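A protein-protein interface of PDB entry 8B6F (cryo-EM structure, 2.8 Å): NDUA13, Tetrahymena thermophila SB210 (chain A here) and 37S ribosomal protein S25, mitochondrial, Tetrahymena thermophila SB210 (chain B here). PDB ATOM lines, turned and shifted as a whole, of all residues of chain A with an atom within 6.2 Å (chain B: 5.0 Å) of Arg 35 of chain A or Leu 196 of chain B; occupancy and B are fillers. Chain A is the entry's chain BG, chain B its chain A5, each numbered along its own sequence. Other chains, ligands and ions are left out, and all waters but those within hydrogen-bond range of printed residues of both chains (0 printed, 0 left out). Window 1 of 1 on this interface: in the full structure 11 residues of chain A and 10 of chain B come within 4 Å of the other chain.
Of chain B, only Arg 192, Gln 193 and Leu 196 come within 4 Å of Arg 35 of chain A. Printed residues of chain B within 4 Å of Phe 39 of chain A: Arg 192. Of the printed residues of chain A, Gln 193 of chain B touches Ala 27 (2.7 Å) and Arg 35 (2.7 Å). Printed residues of chain B within 4 Å of Ala 27 of chain A: Gln 193 (2.7 Å), Leu 196 (3.5 Å), Asp 197 (3.2 Å) and Trp 200 (3.8 Å). Glu 32 of chain A touches none of the printed residues of chain B. Ser 36 of chain A touches none of the printed residues of chain B. The nearest printed residue of chain B that does not touch Arg 35 of chain A is Asp 197 of chain B (7.0 Å). The nearest residue of chain A that does not touch Leu 196 of chain B is Lys 34 of chain A (4.1 Å).
The backbone NH (N) of Ala 27 of chain A sits at hydrogen-bond distance from the side-chain carboxylate (OD1) of Asp 197 of chain B (3.2 Å). NH2 of Arg 35 of chain A sits at hydrogen-bond distance from OE1 of Gln 193 of chain B (2.7 Å). The backbone carbonyl oxygen of Ala 27 of chain A is in hydrogen-bond range of the side-chain amide nitrogen of Gln 193 of chain B. NZ of Lys 34 of chain A is in salt-bridge range of OE1 of Glu 199 of chain B (3.4 Å).
O of Asp 197 of chain B is in hydrogen-bond range of OG1 of Thr 201 of chain B (3.0 Å). OD1 of Asp 197 of chain B lies within hydrogen-bond range of NE2 of Gln 193 of chain B (2.8 Å).
Among the printed residues, merely in contact across the chains: Arg 35 of chain A with Leu 196 of chain B, Leu 38 of chain A with Glu 199 of chain B, Phe 39 of chain A with Arg 192 of chain B, Ala 27 of chain A with Leu 196 of chain B, Ala 27 of chain A with Trp 200 of chain B, Leu 31 of chain A with Leu 196 of chain B, Arg 35 of chain A with Arg 192 of chain B and Leu 38 of chain A with Leu 196 of chain B.
Of the 10 printed residues of chain B, 6 touch a printed residue of chain A. Hydrophobic or aromatic side chains of chain B that line the printed part of chain A: Leu 196 and Trp 200. Along chain B the printed residues that touch a printed residue of chain A span positions 192 to 200. Among the printed residues, 12 pairs touch across the chains.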
ATOM      1  N   ALA A  27       4.366  10.088 -11.630  1.00  0.00           N
ATOM      2  CA  ALA A  27       3.158   9.289 -11.845  1.00  0.00           C
ATOM      3  C   ALA A  27       3.526   8.092 -12.716  1.00  0.00           C
ATOM      4  O   ALA A  27       3.380   8.101 -13.939  1.00  0.00           O
ATOM      5  CB  ALA A  27       2.059  10.132 -12.477  1.00  0.00           C
ATOM      6  N   LEU A  31      -0.947   3.268 -13.221  1.00  0.00           N
ATOM      7  CA  LEU A  31      -1.538   4.289 -14.073  1.00  0.00           C
ATOM      8  C   LEU A  31      -2.315   3.700 -15.243  1.00  0.00           C
ATOM      9  O   LEU A  31      -2.700   4.440 -16.154  1.00  0.00           O
ATOM     10  CB  LEU A  31      -0.451   5.232 -14.594  1.00  0.00           C
ATOM     11  CG  LEU A  31      -0.045   6.412 -13.704  1.00  0.00           C
ATOM     12  CD1 LEU A  31      -1.193   7.395 -13.554  1.00  0.00           C
ATOM     13  CD2 LEU A  31       0.423   5.942 -12.341  1.00  0.00           C
ATOM     14  N   GLU A  32      -2.558   2.388 -15.244  1.00  0.00           N
ATOM     15  CA  GLU A  32      -3.238   1.766 -16.377  1.00  0.00           C
ATOM     16  C   GLU A  32      -4.651   2.313 -16.532  1.00  0.00           C
ATOM     17  O   GLU A  32      -5.043   2.758 -17.616  1.00  0.00           O
ATOM     18  CB  GLU A  32      -3.269   0.245 -16.210  1.00  0.00           C
ATOM     19  CG  GLU A  32      -1.919  -0.438 -16.389  1.00  0.00           C
ATOM     20  CD  GLU A  32      -0.964  -0.176 -15.239  1.00  0.00           C
ATOM     21  OE1 GLU A  32      -1.394   0.430 -14.236  1.00  0.00           O
ATOM     22  OE2 GLU A  32       0.215  -0.577 -15.338  1.00  0.00           O
ATOM     23  N   ASP A  33      -5.435   2.282 -15.453  1.00  0.00           N
ATOM     24  CA  ASP A  33      -6.814   2.748 -15.530  1.00  0.00           C
ATOM     25  C   ASP A  33      -6.874   4.238 -15.839  1.00  0.00           C
ATOM     26  O   ASP A  33      -7.692   4.680 -16.653  1.00  0.00           O
ATOM     27  CB  ASP A  33      -7.535   2.439 -14.219  1.00  0.00           C
ATOM     28  CG  ASP A  33      -9.018   2.746 -14.282  1.00  0.00           C
ATOM     29  OD1 ASP A  33      -9.491   3.192 -15.348  1.00  0.00           O
ATOM     30  OD2 ASP A  33      -9.713   2.539 -13.266  1.00  0.00           O
ATOM     31  N   LYS A  34      -6.013   5.029 -15.194  1.00  0.00           N
ATOM     32  CA  LYS A  34      -6.012   6.468 -15.426  1.00  0.00           C
ATOM     33  C   LYS A  34      -5.665   6.792 -16.873  1.00  0.00           C
ATOM     34  O   LYS A  34      -6.303   7.646 -17.499  1.00  0.00           O
ATOM     35  CB  LYS A  34      -5.032   7.143 -14.470  1.00  0.00           C
ATOM     36  CG  LYS A  34      -5.241   8.637 -14.315  1.00  0.00           C
ATOM     37  CD  LYS A  34      -4.457   9.163 -13.125  1.00  0.00           C
ATOM     38  CE  LYS A  34      -4.767  10.624 -12.857  1.00  0.00           C
ATOM     39  NZ  LYS A  34      -4.132  11.097 -11.598  1.00  0.00           N
ATOM     40  N   ARG A  35      -4.656   6.114 -17.424  1.00  0.00           N
ATOM     41  CA  ARG A  35      -4.287   6.339 -18.817  1.00  0.00           C
ATOM     42  C   ARG A  35      -5.402   5.916 -19.763  1.00  0.00           C
ATOM     43  O   ARG A  35      -5.685   6.607 -20.748  1.00  0.00           O
ATOM     44  CB  ARG A  35      -2.996   5.591 -19.143  1.00  0.00           C
ATOM     45  CG  ARG A  35      -1.760   6.208 -18.519  1.00  0.00           C
ATOM     46  CD  ARG A  35      -0.526   5.368 -18.789  1.00  0.00           C
ATOM     47  NE  ARG A  35       0.689   6.022 -18.319  1.00  0.00           N
ATOM     48  CZ  ARG A  35       1.415   6.871 -19.034  1.00  0.00           C
ATOM     49  NH1 ARG A  35       1.080   7.199 -20.271  1.00  0.00           N
ATOM     50  NH2 ARG A  35       2.504   7.408 -18.491  1.00  0.00           N
ATOM     51  N   SER A  36      -6.046   4.783 -19.485  1.00  0.00           N
ATOM     52  CA  SER A  36      -7.139   4.336 -20.343  1.00  0.00           C
ATOM     53  C   SER A  36      -8.276   5.350 -20.354  1.00  0.00           C
ATOM     54  O   SER A  36      -8.864   5.622 -21.407  1.00  0.00           O
ATOM     55  CB  SER A  36      -7.643   2.969 -19.881  1.00  0.00           C
ATOM     56  OG  SER A  36      -8.261   3.056 -18.608  1.00  0.00           O
ATOM     57  N   LYS A  37      -8.607   5.913 -19.192  1.00  0.00           N
ATOM     58  CA  LYS A  37      -9.652   6.930 -19.141  1.00  0.00           C
ATOM     59  C   LYS A  37      -9.229   8.200 -19.870  1.00  0.00           C
ATOM     60  O   LYS A  37     -10.033   8.806 -20.588  1.00  0.00           O
ATOM     61  CB  LYS A  37     -10.005   7.245 -17.687  1.00  0.00           C
ATOM     62  CG  LYS A  37     -10.831   6.170 -16.999  1.00  0.00           C
ATOM     63  CD  LYS A  37     -11.268   6.619 -15.611  1.00  0.00           C
ATOM     64  CE  LYS A  37     -12.273   5.654 -15.001  1.00  0.00           C
ATOM     65  NZ  LYS A  37     -11.702   4.295 -14.800  1.00  0.00           N
ATOM     66  N   LEU A  38      -7.976   8.621 -19.699  1.00  0.00           N
ATOM     67  CA  LEU A  38      -7.546   9.916 -20.215  1.00  0.00           C
ATOM     68  C   LEU A  38      -7.288   9.908 -21.717  1.00  0.00           C
ATOM     69  O   LEU A  38      -7.476  10.939 -22.370  1.00  0.00           O
ATOM     70  CB  LEU A  38      -6.284  10.383 -19.488  1.00  0.00           C
ATOM     71  CG  LEU A  38      -6.501  11.373 -18.344  1.00  0.00           C
ATOM     72  CD1 LEU A  38      -7.448  10.806 -17.301  1.00  0.00           C
ATOM     73  CD2 LEU A  38      -5.173  11.749 -17.714  1.00  0.00           C
ATOM     74  N   PHE A  39      -6.856   8.789 -22.283  1.00  0.00           N
ATOM     75  CA  PHE A  39      -6.363   8.763 -23.649  1.00  0.00           C
ATOM     76  C   PHE A  39      -7.130   7.757 -24.497  1.00  0.00           C
ATOM     77  O   PHE A  39      -7.717   6.805 -23.972  1.00  0.00           O
ATOM     78  CB  PHE A  39      -4.864   8.429 -23.668  1.00  0.00           C
ATOM     79  CG  PHE A  39      -4.039   9.351 -22.822  1.00  0.00           C
ATOM     80  CD1 PHE A  39      -3.826  10.661 -23.216  1.00  0.00           C
ATOM     81  CD2 PHE A  39      -3.486   8.915 -21.630  1.00  0.00           C
ATOM     82  CE1 PHE A  39      -3.075  11.520 -22.440  1.00  0.00           C
ATOM     83  CE2 PHE A  39      -2.734   9.767 -20.848  1.00  0.00           C
ATOM     84  CZ  PHE A  39      -2.527  11.072 -21.255  1.00  0.00           C
ATOM     85  N   PRO A  40      -7.145   7.941 -25.819  1.00  0.00           N
ATOM     86  CA  PRO A  40      -7.949   7.059 -26.673  1.00  0.00           C
ATOM     87  C   PRO A  40      -7.470   5.617 -26.620  1.00  0.00           C
ATOM     88  O   PRO A  40      -6.286   5.334 -26.425  1.00  0.00           O
ATOM     89  CB  PRO A  40      -7.766   7.654 -28.077  1.00  0.00           C
ATOM     90  CG  PRO A  40      -7.239   9.029 -27.863  1.00  0.00           C
ATOM     91  CD  PRO A  40      -6.444   8.972 -26.604  1.00  0.00           C
ATOM     92  N   ARG B 192       1.804  13.193 -22.243  1.00  0.00           N
ATOM     93  CA  ARG B 192       0.928  12.370 -21.416  1.00  0.00           C
ATOM     94  C   ARG B 192       1.479  12.254 -20.002  1.00  0.00           C
ATOM     95  O   ARG B 192       0.734  12.372 -19.023  1.00  0.00           O
ATOM     96  CB  ARG B 192       0.752  10.986 -22.035  1.00  0.00           C
ATOM     97  CG  ARG B 192       0.203  11.005 -23.445  1.00  0.00           C
ATOM     98  CD  ARG B 192      -0.369   9.650 -23.830  1.00  0.00           C
ATOM     99  NE  ARG B 192       0.656   8.615 -23.895  1.00  0.00           N
ATOM    100  CZ  ARG B 192       1.300   8.255 -24.997  1.00  0.00           C
ATOM    101  NH1 ARG B 192       1.061   8.838 -26.160  1.00  0.00           N
ATOM    102  NH2 ARG B 192       2.204   7.283 -24.932  1.00  0.00           N
ATOM    103  N   GLN B 193       2.788  12.030 -19.877  1.00  0.00           N
ATOM    104  CA  GLN B 193       3.407  11.955 -18.560  1.00  0.00           C
ATOM    105  C   GLN B 193       3.342  13.292 -17.833  1.00  0.00           C
ATOM    106  O   GLN B 193       3.228  13.316 -16.604  1.00  0.00           O
ATOM    107  CB  GLN B 193       4.856  11.490 -18.688  1.00  0.00           C
ATOM    108  CG  GLN B 193       5.494  11.107 -17.367  1.00  0.00           C
ATOM    109  CD  GLN B 193       4.790   9.943 -16.700  1.00  0.00           C
ATOM    110  OE1 GLN B 193       4.332   9.017 -17.365  1.00  0.00           O
ATOM    111  NE2 GLN B 193       4.692   9.992 -15.378  1.00  0.00           N
ATOM    112  N   VAL B 194       3.413  14.405 -18.562  1.00  0.00           N
ATOM    113  CA  VAL B 194       3.272  15.714 -17.926  1.00  0.00           C
ATOM    114  C   VAL B 194       1.883  15.848 -17.314  1.00  0.00           C
ATOM    115  O   VAL B 194       1.732  16.284 -16.167  1.00  0.00           O
ATOM    116  CB  VAL B 194       3.558  16.840 -18.937  1.00  0.00           C
ATOM    117  CG1 VAL B 194       3.189  18.199 -18.356  1.00  0.00           C
ATOM    118  CG2 VAL B 194       5.017  16.830 -19.347  1.00  0.00           C
ATOM    119  N   LYS B 195       0.848  15.475 -18.067  1.00  0.00           N
ATOM    120  CA  LYS B 195      -0.505  15.513 -17.524  1.00  0.00           C
ATOM    121  C   LYS B 195      -0.614  14.641 -16.280  1.00  0.00           C
ATOM    122  O   LYS B 195      -1.176  15.058 -15.261  1.00  0.00           O
ATOM    123  CB  LYS B 195      -1.506  15.046 -18.581  1.00  0.00           C
ATOM    124  CG  LYS B 195      -1.777  16.041 -19.687  1.00  0.00           C
ATOM    125  CD  LYS B 195      -2.808  15.482 -20.657  1.00  0.00           C
ATOM    126  CE  LYS B 195      -3.282  16.536 -21.635  1.00  0.00           C
ATOM    127  NZ  LYS B 195      -4.285  15.991 -22.590  1.00  0.00           N
ATOM    128  N   LEU B 196      -0.088  13.419 -16.352  1.00  0.00           N
ATOM    129  CA  LEU B 196      -0.182  12.502 -15.221  1.00  0.00           C
ATOM    130  C   LEU B 196       0.560  13.044 -14.007  1.00  0.00           C
ATOM    131  O   LEU B 196       0.077  12.932 -12.874  1.00  0.00           O
ATOM    132  CB  LEU B 196       0.361  11.131 -15.617  1.00  0.00           C
ATOM    133  CG  LEU B 196      -0.453  10.384 -16.678  1.00  0.00           C
ATOM    134  CD1 LEU B 196       0.230   9.087 -17.052  1.00  0.00           C
ATOM    135  CD2 LEU B 196      -1.881  10.128 -16.220  1.00  0.00           C
ATOM    136  N   ASP B 197       1.739  13.632 -14.220  1.00  0.00           N
ATOM    137  CA  ASP B 197       2.494  14.193 -13.105  1.00  0.00           C
ATOM    138  C   ASP B 197       1.751  15.356 -12.467  1.00  0.00           C
ATOM    139  O   ASP B 197       1.737  15.492 -11.238  1.00  0.00           O
ATOM    140  CB  ASP B 197       3.876  14.647 -13.576  1.00  0.00           C
ATOM    141  CG  ASP B 197       4.763  13.489 -13.987  1.00  0.00           C
ATOM    142  OD1 ASP B 197       4.305  12.330 -13.915  1.00  0.00           O
ATOM    143  OD2 ASP B 197       5.921  13.739 -14.378  1.00  0.00           O
ATOM    144  N   LEU B 198       1.135  16.213 -13.282  1.00  0.00           N
ATOM    145  CA  LEU B 198       0.368  17.323 -12.729  1.00  0.00           C
ATOM    146  C   LEU B 198      -0.785  16.816 -11.874  1.00  0.00           C
ATOM    147  O   LEU B 198      -1.001  17.294 -10.756  1.00  0.00           O
ATOM    148  CB  LEU B 198      -0.147  18.211 -13.862  1.00  0.00           C
ATOM    149  CG  LEU B 198       0.932  18.951 -14.655  1.00  0.00           C
ATOM    150  CD1 LEU B 198       0.338  19.583 -15.897  1.00  0.00           C
ATOM    151  CD2 LEU B 198       1.607  20.003 -13.796  1.00  0.00           C
ATOM    152  N   GLU B 199      -1.537  15.839 -12.383  1.00  0.00           N
ATOM    153  CA  GLU B 199      -2.654  15.298 -11.614  1.00  0.00           C
ATOM    154  C   GLU B 199      -2.157  14.605 -10.352  1.00  0.00           C
ATOM    155  O   GLU B 199      -2.800  14.676  -9.300  1.00  0.00           O
ATOM    156  CB  GLU B 199      -3.474  14.343 -12.476  1.00  0.00           C
ATOM    157  CG  GLU B 199      -4.102  15.017 -13.683  1.00  0.00           C
ATOM    158  CD  GLU B 199      -5.082  14.125 -14.411  1.00  0.00           C
ATOM    159  OE1 GLU B 199      -5.663  13.227 -13.769  1.00  0.00           O
ATOM    160  OE2 GLU B 199      -5.273  14.325 -15.628  1.00  0.00           O
ATOM    161  N   TRP B 200      -1.018  13.918 -10.445  1.00  0.00           N
ATOM    162  CA  TRP B 200      -0.444  13.268  -9.271  1.00  0.00           C
ATOM    163  C   TRP B 200      -0.065  14.294  -8.211  1.00  0.00           C
ATOM    164  O   TRP B 200      -0.306  14.083  -7.018  1.00  0.00           O
ATOM    165  CB  TRP B 200       0.773  12.437  -9.683  1.00  0.00           C
ATOM    166  CG  TRP B 200       1.474  11.760  -8.543  1.00  0.00           C
ATOM    167  CD1 TRP B 200       1.183  10.538  -8.013  1.00  0.00           C
ATOM    168  CD2 TRP B 200       2.593  12.263  -7.801  1.00  0.00           C
ATOM    169  NE1 TRP B 200       2.047  10.249  -6.985  1.00  0.00           N
ATOM    170  CE2 TRP B 200       2.922  11.292  -6.835  1.00  0.00           C
ATOM    171  CE3 TRP B 200       3.345  13.440  -7.859  1.00  0.00           C
ATOM    172  CZ2 TRP B 200       3.969  11.463  -5.933  1.00  0.00           C
ATOM    173  CZ3 TRP B 200       4.386  13.608  -6.963  1.00  0.00           C
ATOM    174  CH2 TRP B 200       4.688  12.624  -6.012  1.00  0.00           C
ATOM    175  N   THR B 201       0.535  15.411  -8.626  1.00  0.00           N
ATOM    176  CA  THR B 201       0.882  16.459  -7.672  1.00  0.00           C
ATOM    177  C   THR B 201      -0.363  17.036  -7.010  1.00  0.00           C
ATOM    178  O   THR B 201      -0.380  17.262  -5.795  1.00  0.00           O
ATOM    179  CB  THR B 201       1.672  17.565  -8.371  1.00  0.00           C
ATOM    180  OG1 THR B 201       2.876  17.022  -8.926  1.00  0.00           O
ATOM    181  CG2 THR B 201       2.031  18.677  -7.392  1.00  0.00           C
